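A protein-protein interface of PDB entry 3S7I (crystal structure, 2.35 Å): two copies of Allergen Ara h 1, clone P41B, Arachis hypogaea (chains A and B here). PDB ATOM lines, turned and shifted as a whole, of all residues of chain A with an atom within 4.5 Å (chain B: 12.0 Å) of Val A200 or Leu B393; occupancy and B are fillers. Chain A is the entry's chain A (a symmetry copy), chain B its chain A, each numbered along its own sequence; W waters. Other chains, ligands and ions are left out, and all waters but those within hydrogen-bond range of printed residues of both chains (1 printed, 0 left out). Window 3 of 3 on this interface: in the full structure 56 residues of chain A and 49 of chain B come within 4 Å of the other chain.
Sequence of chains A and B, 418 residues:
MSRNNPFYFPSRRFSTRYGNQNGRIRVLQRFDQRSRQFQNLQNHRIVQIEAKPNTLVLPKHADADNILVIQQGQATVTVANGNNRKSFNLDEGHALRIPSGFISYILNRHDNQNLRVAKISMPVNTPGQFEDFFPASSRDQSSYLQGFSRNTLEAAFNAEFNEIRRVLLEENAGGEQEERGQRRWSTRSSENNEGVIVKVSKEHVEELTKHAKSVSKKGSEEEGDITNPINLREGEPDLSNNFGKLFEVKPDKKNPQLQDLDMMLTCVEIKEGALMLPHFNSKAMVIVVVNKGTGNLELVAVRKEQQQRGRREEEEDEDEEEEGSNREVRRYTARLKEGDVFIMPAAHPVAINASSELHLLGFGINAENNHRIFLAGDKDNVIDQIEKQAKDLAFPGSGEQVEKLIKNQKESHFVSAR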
ATOM      1  N   ASN A  54     -14.405  20.927   8.630  1.00  0.00           N
ATOM      2  CA  ASN A  54     -14.952  20.845   7.265  1.00  0.00           C
ATOM      3  C   ASN A  54     -15.507  22.178   6.779  1.00  0.00           C
ATOM      4  O   ASN A  54     -16.620  22.253   6.219  1.00  0.00           O
ATOM      5  CB  ASN A  54     -16.005  19.703   7.169  1.00  0.00           C
ATOM      6  CG  ASN A  54     -15.405  18.317   7.549  1.00  0.00           C
ATOM      7  OD1 ASN A  54     -14.226  18.066   7.266  1.00  0.00           O
ATOM      8  ND2 ASN A  54     -16.179  17.457   8.231  1.00  0.00           N
ATOM      9  N   THR A  55     -14.734  23.222   7.009  1.00  0.00           N
ATOM     10  CA  THR A  55     -15.048  24.556   6.479  1.00  0.00           C
ATOM     11  C   THR A  55     -13.891  25.147   5.731  1.00  0.00           C
ATOM     12  O   THR A  55     -12.782  24.737   5.899  1.00  0.00           O
ATOM     13  CB  THR A  55     -15.510  25.539   7.553  1.00  0.00           C
ATOM     14  OG1 THR A  55     -14.409  25.860   8.441  1.00  0.00           O
ATOM     15  CG2 THR A  55     -16.688  24.928   8.341  1.00  0.00           C
ATOM     16  N   LEU A  56     -14.191  26.074   4.836  1.00  0.00           N
ATOM     17  CA  LEU A  56     -13.171  26.757   4.036  1.00  0.00           C
ATOM     18  C   LEU A  56     -13.401  28.251   4.075  1.00  0.00           C
ATOM     19  O   LEU A  56     -14.534  28.707   3.793  1.00  0.00           O
ATOM     20  CB  LEU A  56     -13.272  26.303   2.595  1.00  0.00           C
ATOM     21  CG  LEU A  56     -12.407  26.911   1.490  1.00  0.00           C
ATOM     22  CD1 LEU A  56     -11.018  26.363   1.661  1.00  0.00           C
ATOM     23  CD2 LEU A  56     -13.008  26.546   0.130  1.00  0.00           C
ATOM     24  N   LEU A  58     -12.976  31.431   2.041  1.00  0.00           N
ATOM     25  CA  LEU A  58     -12.946  31.480   0.571  1.00  0.00           C
ATOM     26  C   LEU A  58     -11.786  32.322   0.064  1.00  0.00           C
ATOM     27  O   LEU A  58     -11.291  33.108   0.782  1.00  0.00           O
ATOM     28  CB  LEU A  58     -14.247  32.026   0.047  1.00  0.00           C
ATOM     29  CG  LEU A  58     -15.423  31.054   0.221  1.00  0.00           C
ATOM     30  CD1 LEU A  58     -16.657  31.833  -0.044  1.00  0.00           C
ATOM     31  CD2 LEU A  58     -15.305  29.844  -0.638  1.00  0.00           C
ATOM     32  N   ASN A 172     -24.650  33.631  -5.105  1.00  0.00           N
ATOM     33  CA  ASN A 172     -24.466  32.189  -4.828  1.00  0.00           C
ATOM     34  C   ASN A 172     -25.076  31.740  -3.495  1.00  0.00           C
ATOM     35  O   ASN A 172     -24.434  31.881  -2.456  1.00  0.00           O
ATOM     36  CB  ASN A 172     -22.958  31.870  -4.860  1.00  0.00           C
ATOM     37  CG  ASN A 172     -22.627  30.408  -4.577  1.00  0.00           C
ATOM     38  OD1 ASN A 172     -21.627  30.120  -3.904  1.00  0.00           O
ATOM     39  ND2 ASN A 172     -23.414  29.489  -5.116  1.00  0.00           N
ATOM     40  N   VAL A 198     -17.384  28.734   4.543  1.00  0.00           N
ATOM     41  CA  VAL A 198     -18.410  27.843   4.070  1.00  0.00           C
ATOM     42  C   VAL A 198     -18.155  26.399   4.475  1.00  0.00           C
ATOM     43  O   VAL A 198     -17.005  25.996   4.694  1.00  0.00           O
ATOM     44  CB  VAL A 198     -18.625  27.931   2.541  1.00  0.00           C
ATOM     45  CG1 VAL A 198     -19.093  29.374   2.115  1.00  0.00           C
ATOM     46  CG2 VAL A 198     -17.420  27.449   1.767  1.00  0.00           C
ATOM     47  N   LYS A 199     -19.267  25.643   4.636  1.00  0.00           N
ATOM     48  CA  LYS A 199     -19.213  24.197   4.920  1.00  0.00           C
ATOM     49  C   LYS A 199     -18.709  23.492   3.686  1.00  0.00           C
ATOM     50  O   LYS A 199     -18.935  23.973   2.589  1.00  0.00           O
ATOM     51  CB  LYS A 199     -20.576  23.649   5.373  1.00  0.00           C
ATOM     52  CG  LYS A 199     -21.139  24.430   6.559  1.00  0.00           C
ATOM     53  CD  LYS A 199     -22.020  23.649   7.471  1.00  0.00           C
ATOM     54  CE  LYS A 199     -23.208  24.501   7.902  1.00  0.00           C
ATOM     55  NZ  LYS A 199     -24.195  24.710   6.751  1.00  0.00           N
ATOM     56  N   VAL A 200     -17.925  22.431   3.860  1.00  0.00           N
ATOM     57  CA  VAL A 200     -17.412  21.658   2.717  1.00  0.00           C
ATOM     58  C   VAL A 200     -17.637  20.139   2.916  1.00  0.00           C
ATOM     59  O   VAL A 200     -17.467  19.615   4.007  1.00  0.00           O
ATOM     60  CB  VAL A 200     -15.949  21.935   2.424  1.00  0.00           C
ATOM     61  CG1 VAL A 200     -15.488  21.132   1.235  1.00  0.00           C
ATOM     62  CG2 VAL A 200     -15.687  23.470   2.202  1.00  0.00           C
ATOM     63  N   SER A 201     -18.038  19.449   1.859  1.00  0.00           N
ATOM     64  CA  SER A 201     -18.369  18.017   1.956  1.00  0.00           C
ATOM     65  C   SER A 201     -17.127  17.239   2.270  1.00  0.00           C
ATOM     66  O   SER A 201     -15.996  17.716   2.027  1.00  0.00           O
ATOM     67  CB  SER A 201     -18.921  17.494   0.640  1.00  0.00           C
ATOM     68  OG  SER A 201     -20.145  18.128   0.372  1.00  0.00           O
ATOM     69  N   LYS A 202     -17.356  16.042   2.810  1.00  0.00           N
ATOM     70  CA  LYS A 202     -16.281  15.144   3.219  1.00  0.00           C
ATOM     71  C   LYS A 202     -15.467  14.808   1.994  1.00  0.00           C
ATOM     72  O   LYS A 202     -14.246  14.764   2.051  1.00  0.00           O
ATOM     73  CB  LYS A 202     -16.850  13.865   3.878  1.00  0.00           C
ATOM     74  CG  LYS A 202     -17.224  14.120   5.333  1.00  0.00           C
ATOM     75  CD  LYS A 202     -17.132  12.835   6.246  1.00  0.00           C
ATOM     76  CE  LYS A 202     -16.607  13.168   7.663  1.00  0.00           C
ATOM     77  NZ  LYS A 202     -15.528  14.194   7.642  1.00  0.00           N
ATOM     78  N   HIS A 204     -15.216  16.639  -0.890  1.00  0.00           N
ATOM     79  CA  HIS A 204     -14.565  17.871  -1.324  1.00  0.00           C
ATOM     80  C   HIS A 204     -13.287  18.189  -0.542  1.00  0.00           C
ATOM     81  O   HIS A 204     -12.294  18.673  -1.115  1.00  0.00           O
ATOM     82  CB  HIS A 204     -15.536  19.056  -1.172  1.00  0.00           C
ATOM     83  CG  HIS A 204     -16.724  19.016  -2.101  1.00  0.00           C
ATOM     84  ND1 HIS A 204     -17.788  19.894  -1.984  1.00  0.00           N
ATOM     85  CD2 HIS A 204     -17.003  18.234  -3.174  1.00  0.00           C
ATOM     86  CE1 HIS A 204     -18.662  19.660  -2.951  1.00  0.00           C
ATOM     87  NE2 HIS A 204     -18.222  18.641  -3.675  1.00  0.00           N
ATOM     88  N   VAL A 205     -13.332  17.971   0.775  1.00  0.00           N
ATOM     89  CA  VAL A 205     -12.153  18.119   1.639  1.00  0.00           C
ATOM     90  C   VAL A 205     -11.106  17.125   1.164  1.00  0.00           C
ATOM     91  O   VAL A 205      -9.939  17.436   1.113  1.00  0.00           O
ATOM     92  CB  VAL A 205     -12.462  17.870   3.141  1.00  0.00           C
ATOM     93  CG1 VAL A 205     -11.143  17.858   4.011  1.00  0.00           C
ATOM     94  CG2 VAL A 205     -13.524  18.870   3.675  1.00  0.00           C
ATOM     95  N   LEU A 208      -9.646  18.716  -1.952  1.00  0.00           N
ATOM     96  CA  LEU A 208      -8.906  19.976  -1.698  1.00  0.00           C
ATOM     97  C   LEU A 208      -7.571  19.722  -1.051  1.00  0.00           C
ATOM     98  O   LEU A 208      -6.721  20.612  -1.012  1.00  0.00           O
ATOM     99  CB  LEU A 208      -9.702  20.921  -0.787  1.00  0.00           C
ATOM    100  CG  LEU A 208     -10.922  21.617  -1.378  1.00  0.00           C
ATOM    101  CD1 LEU A 208     -11.863  22.178  -0.346  1.00  0.00           C
ATOM    102  CD2 LEU A 208     -10.486  22.708  -2.339  1.00  0.00           C
ATOM    103  N   ILE B 383      -7.148  33.809 -11.187  1.00  0.00           N
ATOM    104  CA  ILE B 383      -8.411  33.111 -10.994  1.00  0.00           C
ATOM    105  C   ILE B 383      -8.331  31.687 -11.569  1.00  0.00           C
ATOM    106  O   ILE B 383      -8.654  30.717 -10.883  1.00  0.00           O
ATOM    107  CB  ILE B 383      -9.516  33.889 -11.620  1.00  0.00           C
ATOM    108  CG1 ILE B 383      -9.591  35.280 -10.940  1.00  0.00           C
ATOM    109  CG2 ILE B 383     -10.780  33.122 -11.548  1.00  0.00           C
ATOM    110  CD1 ILE B 383     -10.774  36.123 -11.389  1.00  0.00           C
ATOM    111  N   ILE B 386      -6.875  29.260  -9.058  1.00  0.00           N
ATOM    112  CA  ILE B 386      -7.669  28.728  -7.933  1.00  0.00           C
ATOM    113  C   ILE B 386      -8.067  27.286  -8.198  1.00  0.00           C
ATOM    114  O   ILE B 386      -8.462  26.950  -9.320  1.00  0.00           O
ATOM    115  CB  ILE B 386      -8.986  29.544  -7.707  1.00  0.00           C
ATOM    116  CG1 ILE B 386      -8.616  31.038  -7.399  1.00  0.00           C
ATOM    117  CG2 ILE B 386      -9.884  28.854  -6.635  1.00  0.00           C
ATOM    118  CD1 ILE B 386      -9.806  32.028  -7.287  1.00  0.00           C
ATOM    119  N   GLU B 387      -8.018  26.420  -7.194  1.00  0.00           N
ATOM    120  CA  GLU B 387      -8.458  25.006  -7.462  1.00  0.00           C
ATOM    121  C   GLU B 387      -9.897  24.946  -7.881  1.00  0.00           C
ATOM    122  O   GLU B 387     -10.728  25.741  -7.446  1.00  0.00           O
ATOM    123  CB  GLU B 387      -8.252  24.098  -6.307  1.00  0.00           C
ATOM    124  CG  GLU B 387      -6.830  23.605  -6.167  1.00  0.00           C
ATOM    125  CD  GLU B 387      -6.400  23.359  -4.691  1.00  0.00           C
ATOM    126  OE1 GLU B 387      -6.140  22.194  -4.345  1.00  0.00           O
ATOM    127  OE2 GLU B 387      -6.278  24.341  -3.907  1.00  0.00           O
ATOM    128  N   LYS B 388     -10.192  23.947  -8.705  1.00  0.00           N
ATOM    129  CA  LYS B 388     -11.485  23.801  -9.297  1.00  0.00           C
ATOM    130  C   LYS B 388     -12.492  23.720  -8.197  1.00  0.00           C
ATOM    131  O   LYS B 388     -13.508  24.432  -8.226  1.00  0.00           O
ATOM    132  CB  LYS B 388     -11.498  22.545 -10.117  1.00  0.00           C
ATOM    133  CG  LYS B 388     -12.577  22.524 -11.170  1.00  0.00           C
ATOM    134  CD  LYS B 388     -13.077  21.098 -11.383  1.00  0.00           C
ATOM    135  CE  LYS B 388     -13.709  20.996 -12.695  1.00  0.00           C
ATOM    136  NZ  LYS B 388     -13.856  19.607 -13.055  1.00  0.00           N
ATOM    137  N   GLN B 389     -12.202  22.868  -7.215  1.00  0.00           N
ATOM    138  CA  GLN B 389     -13.115  22.658  -6.159  1.00  0.00           C
ATOM    139  C   GLN B 389     -13.338  23.927  -5.382  1.00  0.00           C
ATOM    140  O   GLN B 389     -14.452  24.159  -4.911  1.00  0.00           O
ATOM    141  CB  GLN B 389     -12.634  21.564  -5.223  1.00  0.00           C
ATOM    142  CG  GLN B 389     -13.638  21.301  -4.121  1.00  0.00           C
ATOM    143  CD  GLN B 389     -14.975  20.736  -4.647  1.00  0.00           C
ATOM    144  OE1 GLN B 389     -15.034  19.578  -5.047  1.00  0.00           O
ATOM    145  NE2 GLN B 389     -16.045  21.548  -4.617  1.00  0.00           N
ATOM    146  N   ALA B 390     -12.285  24.719  -5.185  1.00  0.00           N
ATOM    147  CA  ALA B 390     -12.449  26.027  -4.564  1.00  0.00           C
ATOM    148  C   ALA B 390     -13.198  27.018  -5.468  1.00  0.00           C
ATOM    149  O   ALA B 390     -13.939  27.868  -4.973  1.00  0.00           O
ATOM    150  CB  ALA B 390     -11.098  26.600  -4.117  1.00  0.00           C
ATOM    151  N   LYS B 391     -13.012  26.938  -6.780  1.00  0.00           N
ATOM    152  CA  LYS B 391     -13.856  27.712  -7.675  1.00  0.00           C
ATOM    153  C   LYS B 391     -15.344  27.350  -7.474  1.00  0.00           C
ATOM    154  O   LYS B 391     -16.226  28.230  -7.402  1.00  0.00           O
ATOM    155  CB  LYS B 391     -13.419  27.534  -9.135  1.00  0.00           C
ATOM    156  CG  LYS B 391     -11.909  27.899  -9.355  1.00  0.00           C
ATOM    157  CD  LYS B 391     -11.571  28.500 -10.763  1.00  0.00           C
ATOM    158  CE  LYS B 391     -10.814  27.531 -11.718  1.00  0.00           C
ATOM    159  NZ  LYS B 391      -9.313  27.635 -11.782  1.00  0.00           N
ATOM    160  N   ASP B 392     -15.612  26.053  -7.331  1.00  0.00           N
ATOM    161  CA  ASP B 392     -16.975  25.588  -7.194  1.00  0.00           C
ATOM    162  C   ASP B 392     -17.666  26.128  -5.940  1.00  0.00           C
ATOM    163  O   ASP B 392     -18.852  26.419  -5.953  1.00  0.00           O
ATOM    164  CB  ASP B 392     -17.008  24.067  -7.102  1.00  0.00           C
ATOM    165  CG  ASP B 392     -18.410  23.542  -7.029  1.00  0.00           C
ATOM    166  OD1 ASP B 392     -19.147  23.741  -8.028  1.00  0.00           O
ATOM    167  OD2 ASP B 392     -18.782  22.893  -6.008  1.00  0.00           O
ATOM    168  N   LEU B 393     -16.920  26.175  -4.850  1.00  0.00           N
ATOM    169  CA  LEU B 393     -17.423  26.635  -3.570  1.00  0.00           C
ATOM    170  C   LEU B 393     -17.652  28.170  -3.444  1.00  0.00           C
ATOM    171  O   LEU B 393     -18.525  28.627  -2.659  1.00  0.00           O
ATOM    172  CB  LEU B 393     -16.445  26.189  -2.459  1.00  0.00           C
ATOM    173  CG  LEU B 393     -16.482  24.678  -2.164  1.00  0.00           C
ATOM    174  CD1 LEU B 393     -15.469  24.299  -1.190  1.00  0.00           C
ATOM    175  CD2 LEU B 393     -17.895  24.180  -1.706  1.00  0.00           C
ATOM    176  N   ALA B 394     -16.875  28.948  -4.190  1.00  0.00           N
ATOM    177  CA  ALA B 394     -16.893  30.369  -4.048  1.00  0.00           C
ATOM    178  C   ALA B 394     -17.820  31.021  -5.049  1.00  0.00           C
ATOM    179  O   ALA B 394     -18.647  31.858  -4.682  1.00  0.00           O
ATOM    180  CB  ALA B 394     -15.501  30.885  -4.224  1.00  0.00           C
ATOM    181  N   PHE B 395     -17.713  30.623  -6.316  1.00  0.00           N
ATOM    182  CA  PHE B 395     -18.570  31.195  -7.332  1.00  0.00           C
ATOM    183  C   PHE B 395     -19.935  30.505  -7.410  1.00  0.00           C
ATOM    184  O   PHE B 395     -20.128  29.409  -6.886  1.00  0.00           O
ATOM    185  CB  PHE B 395     -17.879  31.199  -8.703  1.00  0.00           C
ATOM    186  CG  PHE B 395     -16.521  31.884  -8.728  1.00  0.00           C
ATOM    187  CD1 PHE B 395     -15.343  31.140  -8.700  1.00  0.00           C
ATOM    188  CD2 PHE B 395     -16.424  33.257  -8.848  1.00  0.00           C
ATOM    189  CE1 PHE B 395     -14.104  31.751  -8.788  1.00  0.00           C
ATOM    190  CE2 PHE B 395     -15.167  33.914  -8.955  1.00  0.00           C
ATOM    191  CZ  PHE B 395     -14.003  33.174  -8.930  1.00  0.00           C
ATOM    192  N   PRO B 396     -20.911  31.173  -8.037  1.00  0.00           N
ATOM    193  CA  PRO B 396     -22.238  30.557  -8.277  1.00  0.00           C
ATOM    194  C   PRO B 396     -22.247  29.366  -9.253  1.00  0.00           C
ATOM    195  O   PRO B 396     -23.012  28.430  -9.093  1.00  0.00           O
ATOM    196  CB  PRO B 396     -23.068  31.699  -8.899  1.00  0.00           C
ATOM    197  CG  PRO B 396     -22.296  32.943  -8.622  1.00  0.00           C
ATOM    198  CD  PRO B 396     -20.877  32.618  -8.324  1.00  0.00           C
ATOM    199  N   GLY B 397     -21.462  29.471 -10.317  1.00  0.00           N
ATOM    200  CA  GLY B 397     -21.347  28.401 -11.278  1.00  0.00           C
ATOM    201  C   GLY B 397     -20.588  27.257 -10.689  1.00  0.00           C
ATOM    202  O   GLY B 397     -19.906  27.425  -9.694  1.00  0.00           O
ATOM    203  N   SER B 398     -20.678  26.093 -11.319  1.00  0.00           N
ATOM    204  CA  SER B 398     -19.814  24.963 -10.943  1.00  0.00           C
ATOM    205  C   SER B 398     -18.329  25.278 -11.239  1.00  0.00           C
ATOM    206  O   SER B 398     -18.020  26.200 -11.945  1.00  0.00           O
ATOM    207  CB  SER B 398     -20.224  23.699 -11.686  1.00  0.00           C
ATOM    208  OG  SER B 398     -20.293  23.933 -13.115  1.00  0.00           O
ATOM    209  N   GLY B 399     -17.432  24.461 -10.726  1.00  0.00           N
ATOM    210  CA  GLY B 399     -16.055  24.524 -11.110  1.00  0.00           C
ATOM    211  C   GLY B 399     -15.851  24.390 -12.603  1.00  0.00           C
ATOM    212  O   GLY B 399     -15.011  25.109 -13.150  1.00  0.00           O
ATOM    213  N   GLU B 400     -16.597  23.473 -13.253  1.00  0.00           N
ATOM    214  CA  GLU B 400     -16.524  23.245 -14.704  1.00  0.00           C
ATOM    215  C   GLU B 400     -16.920  24.461 -15.521  1.00  0.00           C
ATOM    216  O   GLU B 400     -16.252  24.781 -16.526  1.00  0.00           O
ATOM    217  CB  GLU B 400     -17.434  22.064 -15.182  1.00  0.00           C
ATOM    218  CG  GLU B 400     -16.879  20.670 -14.826  1.00  0.00           C
ATOM    219  CD  GLU B 400     -17.641  19.532 -15.426  1.00  0.00           C
ATOM    220  OE1 GLU B 400     -18.017  18.596 -14.663  1.00  0.00           O
ATOM    221  OE2 GLU B 400     -17.857  19.539 -16.661  1.00  0.00           O
ATOM    222  N   GLN B 401     -18.010  25.107 -15.099  1.00  0.00           N
ATOM    223  CA  GLN B 401     -18.555  26.276 -15.809  1.00  0.00           C
ATOM    224  C   GLN B 401     -17.514  27.381 -15.722  1.00  0.00           C
ATOM    225  O   GLN B 401     -17.066  27.920 -16.720  1.00  0.00           O
ATOM    226  CB  GLN B 401     -19.882  26.753 -15.169  1.00  0.00           C
ATOM    227  CG  GLN B 401     -21.157  25.967 -15.577  1.00  0.00           C
ATOM    228  CD  GLN B 401     -22.404  26.393 -14.763  1.00  0.00           C
ATOM    229  OE1 GLN B 401     -22.423  26.259 -13.525  1.00  0.00           O
ATOM    230  NE2 GLN B 401     -23.460  26.895 -15.462  1.00  0.00           N
ATOM    231  N   VAL B 402     -17.125  27.673 -14.490  1.00  0.00           N
ATOM    232  CA  VAL B 402     -16.112  28.649 -14.179  1.00  0.00           C
ATOM    233  C   VAL B 402     -14.898  28.500 -15.062  1.00  0.00           C
ATOM    234  O   VAL B 402     -14.582  29.439 -15.797  1.00  0.00           O
ATOM    235  CB  VAL B 402     -15.745  28.574 -12.735  1.00  0.00           C
ATOM    236  CG1 VAL B 402     -14.474  29.383 -12.459  1.00  0.00           C
ATOM    237  CG2 VAL B 402     -16.907  29.134 -11.945  1.00  0.00           C
ATOM    238  N   GLU B 403     -14.276  27.323 -15.026  1.00  0.00           N
ATOM    239  CA  GLU B 403     -13.129  26.977 -15.885  1.00  0.00           C
ATOM    240  C   GLU B 403     -13.416  27.095 -17.384  1.00  0.00           C
ATOM    241  O   GLU B 403     -12.550  27.480 -18.178  1.00  0.00           O
ATOM    242  CB  GLU B 403     -12.595  25.568 -15.543  1.00  0.00           C
ATOM    243  CG  GLU B 403     -11.953  25.531 -14.154  1.00  0.00           C
ATOM    244  CD  GLU B 403     -10.999  24.377 -13.908  1.00  0.00           C
ATOM    245  OE1 GLU B 403     -10.208  24.450 -12.900  1.00  0.00           O
ATOM    246  OE2 GLU B 403     -11.031  23.401 -14.664  1.00  0.00           O
ATOM    247  N   ILE B 406     -13.723  30.876 -18.059  1.00  0.00           N
ATOM    248  CA  ILE B 406     -12.394  31.508 -17.974  1.00  0.00           C
ATOM    249  C   ILE B 406     -11.522  31.253 -19.190  1.00  0.00           C
ATOM    250  O   ILE B 406     -10.640  32.064 -19.482  1.00  0.00           O
ATOM    251  CB  ILE B 406     -11.633  30.970 -16.785  1.00  0.00           C
ATOM    252  CG1 ILE B 406     -11.887  31.844 -15.560  1.00  0.00           C
ATOM    253  CG2 ILE B 406     -10.156  30.837 -17.113  1.00  0.00           C
ATOM    254  CD1 ILE B 406     -11.766  31.047 -14.347  1.00  0.00           C
HETATM  255  O   HOH W   1      -6.652  23.128  -1.157  1.00  0.00           O
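The side-chain carboxylate (OD2) of Asp B392 sits at hydrogen-bond distance from the side-chain amide nitrogen (NE2) of Gln B389, 3.4 Å away.
The backbone NH (N) of Leu A56 sits at hydrogen-bond distance from the backbone carbonyl oxygen (O) of Val A198 (2.8 Å).
The backbone NH (N) of Val A200 sits at hydrogen-bond distance from the backbone carbonyl oxygen (O) of Asn A54 (2.7 Å).
Hydrophobic or aromatic side chains of chain A within 4 Å of the printed part of chain B: Leu A56, Leu A58, Val A200, His A204 and Leu A208.
Among the printed residues, 12 pairs touch across the chains.
Among the printed residues, no Asp or Glu carboxylate lies within 4 Å of a Lys or Arg side-chain nitrogen of the other chain.
Water W1 lies within hydrogen-bond range of the backbone carbonyl oxygen of Leu A208 (2.5 Å) and the side-chain carboxylate of Glu B387 (3.0 Å).
The backbone carbonyl oxygen (O) of Phe B395 sits close to the side-chain amide oxygen (OD1) of Asn A172 (3.4 Å).
No residue of chain B comes within 4 Å of Asn A54.
Of the printed residues of chain B, Leu A58 touches Leu B393 (3.99 Å) and Ala B394 (3.7 Å).
Printed residues of chain B within 4 Å of Asn A172: Leu B393 (3.7 Å), Ala B394 (3.5 Å), Phe B395 (3.4 Å) and Pro B396 (3.5 Å).
No residue of chain B comes within 4 Å of Val A198.
No residue of chain B comes within 4 Å of Lys A199.
Val A200 touches just one residue of chain B: Leu B393 (3.5 Å).
No residue of chain B comes within 4 Å of Lys A202.
His A204 touches just one residue of chain B: Gln B389 (3.0 Å).
Of the printed residues of chain B, Leu A208 touches Glu B387 (3.7 Å), Gln B389 (3.8 Å) and Ala B390 (3.9 Å).
Lys B391 touches none of the printed residues of chain A.
Printed residues of chain A within 4 Å of Leu B393: Leu A56 (3.6 Å), Leu A58 (3.99 Å), Asn A172 (3.7 Å) and Val A200 (3.5 Å).
Printed residues of chain A within 4 Å of Pro B396: Asn A172.
The nearest printed residue of chain A that does not touch Leu B393 is Leu A208 (4.3 Å).
The nearest printed residue of chain A that does not touch Ala B394 is Val A198 (6.2 Å).
Among the printed residues, pairs that only touch across the chains: Leu A56 with Leu B393, Leu A58 with Leu B393, Leu A58 with Ala B394, Asn A172 with Leu B393, Asn A172 with Ala B394, Asn A172 with Pro B396, Val A200 with Leu B393, His A204 with Gln B389, Leu A208 with Glu B387, Leu A208 with Gln B389 and Leu A208 with Ala B390.
No position is printed for both chains.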
